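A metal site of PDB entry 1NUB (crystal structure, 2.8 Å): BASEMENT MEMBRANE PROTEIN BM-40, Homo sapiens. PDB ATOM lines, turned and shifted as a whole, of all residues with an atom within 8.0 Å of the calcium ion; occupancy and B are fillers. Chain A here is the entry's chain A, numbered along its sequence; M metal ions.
The backbone NH (N) of His 167 sits close to the side-chain carboxylate (OE2) of Glu 177 (2.9 Å). OE2 of Glu 177 sits close to N of Gln 166, 3.0 Å away. The backbone NH (N) of Glu 177 lies close to the side-chain hydroxyl (OG) of Ser 174. The side-chain carboxylate (OD2) of Asp 165 sits at hydrogen-bond distance from the backbone NH (N) of Gly 171, at 2.9 Å.
Within 4 Å of the calcium ion: Asp 165, Pro 168, Asp 170, Tyr 172 and Glu 177.
The calcium ion is bound by the side-chain carboxylate (OE1) of Glu 177 (2.3 Å), the backbone carbonyl oxygen (O) of Pro 168 (2.4 Å), the side-chain carboxylate (OE2) of Glu 177 (2.4 Å), the backbone carbonyl oxygen (O) of Tyr 172 (2.6 Å), the side-chain carboxylate (OD1) of Asp 170 (2.6 Å) and the side-chain carboxylate (OD1) of Asp 165 (2.7 Å). The calcium ion has six donor atoms within binding distance.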
ATOM      1  N   PHE A 161     -15.909 -37.094 -18.863  1.00  0.00           N
ATOM      2  CA  PHE A 161     -15.527 -36.183 -17.792  1.00  0.00           C
ATOM      3  C   PHE A 161     -14.127 -35.655 -18.030  1.00  0.00           C
ATOM      4  O   PHE A 161     -13.909 -34.452 -18.036  1.00  0.00           O
ATOM      5  CB  PHE A 161     -15.594 -36.863 -16.419  1.00  0.00           C
ATOM      6  CG  PHE A 161     -15.349 -35.913 -15.278  1.00  0.00           C
ATOM      7  CD1 PHE A 161     -16.402 -35.242 -14.684  1.00  0.00           C
ATOM      8  CD2 PHE A 161     -14.066 -35.706 -14.789  1.00  0.00           C
ATOM      9  CE1 PHE A 161     -16.183 -34.365 -13.640  1.00  0.00           C
ATOM     10  CE2 PHE A 161     -13.838 -34.821 -13.737  1.00  0.00           C
ATOM     11  CZ  PHE A 161     -14.897 -34.162 -13.163  1.00  0.00           C
ATOM     12  N   LEU A 164     -13.821 -33.109 -20.840  1.00  0.00           N
ATOM     13  CA  LEU A 164     -14.327 -31.793 -20.460  1.00  0.00           C
ATOM     14  C   LEU A 164     -13.481 -31.063 -19.416  1.00  0.00           C
ATOM     15  O   LEU A 164     -13.273 -29.849 -19.526  1.00  0.00           O
ATOM     16  CB  LEU A 164     -15.778 -31.873 -19.978  1.00  0.00           C
ATOM     17  CG  LEU A 164     -16.827 -32.361 -20.999  1.00  0.00           C
ATOM     18  CD1 LEU A 164     -18.188 -32.352 -20.372  1.00  0.00           C
ATOM     19  CD2 LEU A 164     -16.829 -31.475 -22.204  1.00  0.00           C
ATOM     20  N   ASP A 165     -12.997 -31.803 -18.419  1.00  0.00           N
ATOM     21  CA  ASP A 165     -12.172 -31.248 -17.352  1.00  0.00           C
ATOM     22  C   ASP A 165     -10.815 -30.784 -17.900  1.00  0.00           C
ATOM     23  O   ASP A 165      -9.798 -31.470 -17.779  1.00  0.00           O
ATOM     24  CB  ASP A 165     -11.984 -32.306 -16.243  1.00  0.00           C
ATOM     25  CG  ASP A 165     -11.194 -31.788 -15.042  1.00  0.00           C
ATOM     26  OD1 ASP A 165     -11.256 -30.586 -14.716  1.00  0.00           O
ATOM     27  OD2 ASP A 165     -10.525 -32.611 -14.385  1.00  0.00           O
ATOM     28  N   GLN A 166     -10.821 -29.612 -18.537  1.00  0.00           N
ATOM     29  CA  GLN A 166      -9.609 -29.063 -19.118  1.00  0.00           C
ATOM     30  C   GLN A 166      -9.222 -27.673 -18.626  1.00  0.00           C
ATOM     31  O   GLN A 166      -8.066 -27.426 -18.294  1.00  0.00           O
ATOM     32  CB  GLN A 166      -9.720 -29.005 -20.647  1.00  0.00           C
ATOM     33  CG  GLN A 166      -9.884 -30.356 -21.329  1.00  0.00           C
ATOM     34  CD  GLN A 166      -8.727 -31.273 -21.067  1.00  0.00           C
ATOM     35  OE1 GLN A 166      -7.561 -30.891 -21.213  1.00  0.00           O
ATOM     36  NE2 GLN A 166      -9.029 -32.496 -20.670  1.00  0.00           N
ATOM     37  N   HIS A 167     -10.175 -26.756 -18.571  1.00  0.00           N
ATOM     38  CA  HIS A 167      -9.872 -25.386 -18.153  1.00  0.00           C
ATOM     39  C   HIS A 167     -10.440 -24.949 -16.814  1.00  0.00           C
ATOM     40  O   HIS A 167     -11.471 -24.283 -16.764  1.00  0.00           O
ATOM     41  CB  HIS A 167     -10.315 -24.386 -19.227  1.00  0.00           C
ATOM     42  CG  HIS A 167     -10.787 -25.025 -20.503  1.00  0.00           C
ATOM     43  ND1 HIS A 167      -9.920 -25.399 -21.508  1.00  0.00           N
ATOM     44  CD2 HIS A 167     -12.023 -25.356 -20.917  1.00  0.00           C
ATOM     45  CE1 HIS A 167     -10.608 -25.943 -22.493  1.00  0.00           C
ATOM     46  NE2 HIS A 167     -11.886 -25.932 -22.160  1.00  0.00           N
ATOM     47  N   PRO A 168      -9.744 -25.277 -15.713  1.00  0.00           N
ATOM     48  CA  PRO A 168      -8.488 -26.035 -15.679  1.00  0.00           C
ATOM     49  C   PRO A 168      -8.737 -27.476 -15.243  1.00  0.00           C
ATOM     50  O   PRO A 168      -9.795 -27.801 -14.730  1.00  0.00           O
ATOM     51  CB  PRO A 168      -7.696 -25.280 -14.618  1.00  0.00           C
ATOM     52  CG  PRO A 168      -8.708 -24.992 -13.611  1.00  0.00           C
ATOM     53  CD  PRO A 168      -9.944 -24.571 -14.437  1.00  0.00           C
ATOM     54  N   ILE A 169      -7.765 -28.343 -15.478  1.00  0.00           N
ATOM     55  CA  ILE A 169      -7.873 -29.739 -15.091  1.00  0.00           C
ATOM     56  C   ILE A 169      -7.779 -29.749 -13.559  1.00  0.00           C
ATOM     57  O   ILE A 169      -6.688 -29.648 -13.004  1.00  0.00           O
ATOM     58  CB  ILE A 169      -6.705 -30.557 -15.701  1.00  0.00           C
ATOM     59  CG1 ILE A 169      -6.649 -30.290 -17.206  1.00  0.00           C
ATOM     60  CG2 ILE A 169      -6.900 -32.037 -15.483  1.00  0.00           C
ATOM     61  CD1 ILE A 169      -5.434 -30.886 -17.878  1.00  0.00           C
ATOM     62  N   ASP A 170      -8.936 -29.768 -12.897  1.00  0.00           N
ATOM     63  CA  ASP A 170      -8.999 -29.738 -11.432  1.00  0.00           C
ATOM     64  C   ASP A 170      -9.884 -30.817 -10.833  1.00  0.00           C
ATOM     65  O   ASP A 170      -9.897 -31.018  -9.607  1.00  0.00           O
ATOM     66  CB  ASP A 170      -9.451 -28.354 -10.947  1.00  0.00           C
ATOM     67  CG  ASP A 170     -10.838 -27.980 -11.442  1.00  0.00           C
ATOM     68  OD1 ASP A 170     -11.409 -28.706 -12.292  1.00  0.00           O
ATOM     69  OD2 ASP A 170     -11.372 -26.955 -10.971  1.00  0.00           O
ATOM     70  N   GLY A 171     -10.647 -31.501 -11.666  1.00  0.00           N
ATOM     71  CA  GLY A 171     -11.507 -32.556 -11.176  1.00  0.00           C
ATOM     72  C   GLY A 171     -12.954 -32.142 -11.072  1.00  0.00           C
ATOM     73  O   GLY A 171     -13.785 -32.916 -10.584  1.00  0.00           O
ATOM     74  N   TYR A 172     -13.252 -30.915 -11.499  1.00  0.00           N
ATOM     75  CA  TYR A 172     -14.619 -30.387 -11.474  1.00  0.00           C
ATOM     76  C   TYR A 172     -14.909 -29.777 -12.833  1.00  0.00           C
ATOM     77  O   TYR A 172     -14.005 -29.366 -13.541  1.00  0.00           O
ATOM     78  CB  TYR A 172     -14.747 -29.297 -10.409  1.00  0.00           C
ATOM     79  CG  TYR A 172     -14.307 -29.699  -9.030  1.00  0.00           C
ATOM     80  CD1 TYR A 172     -12.989 -29.543  -8.630  1.00  0.00           C
ATOM     81  CD2 TYR A 172     -15.217 -30.250  -8.124  1.00  0.00           C
ATOM     82  CE1 TYR A 172     -12.564 -29.920  -7.363  1.00  0.00           C
ATOM     83  CE2 TYR A 172     -14.798 -30.636  -6.856  1.00  0.00           C
ATOM     84  CZ  TYR A 172     -13.476 -30.474  -6.479  1.00  0.00           C
ATOM     85  OH  TYR A 172     -13.065 -30.857  -5.228  1.00  0.00           O
ATOM     86  N   LEU A 173     -16.177 -29.743 -13.201  1.00  0.00           N
ATOM     87  CA  LEU A 173     -16.553 -29.147 -14.476  1.00  0.00           C
ATOM     88  C   LEU A 173     -17.372 -27.890 -14.190  1.00  0.00           C
ATOM     89  O   LEU A 173     -18.342 -27.923 -13.417  1.00  0.00           O
ATOM     90  CB  LEU A 173     -17.376 -30.120 -15.327  1.00  0.00           C
ATOM     91  CG  LEU A 173     -16.741 -31.471 -15.649  1.00  0.00           C
ATOM     92  CD1 LEU A 173     -17.689 -32.290 -16.489  1.00  0.00           C
ATOM     93  CD2 LEU A 173     -15.441 -31.254 -16.366  1.00  0.00           C
ATOM     94  N   SER A 174     -16.914 -26.781 -14.740  1.00  0.00           N
ATOM     95  CA  SER A 174     -17.594 -25.512 -14.562  1.00  0.00           C
ATOM     96  C   SER A 174     -18.613 -25.330 -15.685  1.00  0.00           C
ATOM     97  O   SER A 174     -18.609 -26.076 -16.673  1.00  0.00           O
ATOM     98  CB  SER A 174     -16.573 -24.378 -14.574  1.00  0.00           C
ATOM     99  OG  SER A 174     -15.925 -24.287 -15.833  1.00  0.00           O
ATOM    100  N   GLU A 177     -16.879 -25.299 -18.880  1.00  0.00           N
ATOM    101  CA  GLU A 177     -16.393 -26.599 -19.316  1.00  0.00           C
ATOM    102  C   GLU A 177     -17.460 -27.513 -19.901  1.00  0.00           C
ATOM    103  O   GLU A 177     -17.153 -28.394 -20.703  1.00  0.00           O
ATOM    104  CB  GLU A 177     -15.641 -27.281 -18.183  1.00  0.00           C
ATOM    105  CG  GLU A 177     -14.392 -26.494 -17.787  1.00  0.00           C
ATOM    106  CD  GLU A 177     -13.587 -27.172 -16.711  1.00  0.00           C
ATOM    107  OE1 GLU A 177     -14.102 -27.262 -15.581  1.00  0.00           O
ATOM    108  OE2 GLU A 177     -12.446 -27.580 -17.005  1.00  0.00           O
ATOM    109  N   TYR A 206     -19.955 -26.571  -9.438  1.00  0.00           N
ATOM    110  CA  TYR A 206     -18.983 -27.420 -10.115  1.00  0.00           C
ATOM    111  C   TYR A 206     -19.491 -28.843 -10.022  1.00  0.00           C
ATOM    112  O   TYR A 206     -20.083 -29.233  -9.024  1.00  0.00           O
ATOM    113  CB  TYR A 206     -17.628 -27.342  -9.419  1.00  0.00           C
ATOM    114  CG  TYR A 206     -16.916 -26.037  -9.577  1.00  0.00           C
ATOM    115  CD1 TYR A 206     -17.139 -24.991  -8.695  1.00  0.00           C
ATOM    116  CD2 TYR A 206     -16.027 -25.833 -10.625  1.00  0.00           C
ATOM    117  CE1 TYR A 206     -16.502 -23.770  -8.851  1.00  0.00           C
ATOM    118  CE2 TYR A 206     -15.379 -24.622 -10.798  1.00  0.00           C
ATOM    119  CZ  TYR A 206     -15.621 -23.597  -9.898  1.00  0.00           C
ATOM    120  OH  TYR A 206     -14.986 -22.389 -10.065  1.00  0.00           O
ATOM    121  N   ILE A 207     -19.320 -29.614 -11.092  1.00  0.00           N
ATOM    122  CA  ILE A 207     -19.730 -31.003 -11.063  1.00  0.00           C
ATOM    123  C   ILE A 207     -18.477 -31.825 -10.802  1.00  0.00           C
ATOM    124  O   ILE A 207     -17.528 -31.760 -11.605  1.00  0.00           O
ATOM    125  CB  ILE A 207     -20.371 -31.443 -12.369  1.00  0.00           C
ATOM    126  CG1 ILE A 207     -21.581 -30.547 -12.674  1.00  0.00           C
ATOM    127  CG2 ILE A 207     -20.758 -32.910 -12.293  1.00  0.00           C
ATOM    128  CD1 ILE A 207     -22.587 -30.443 -11.536  1.00  0.00           C
HETATM  129 CA    CA M   1     -12.151 -28.003 -14.661  1.00  0.00          CA
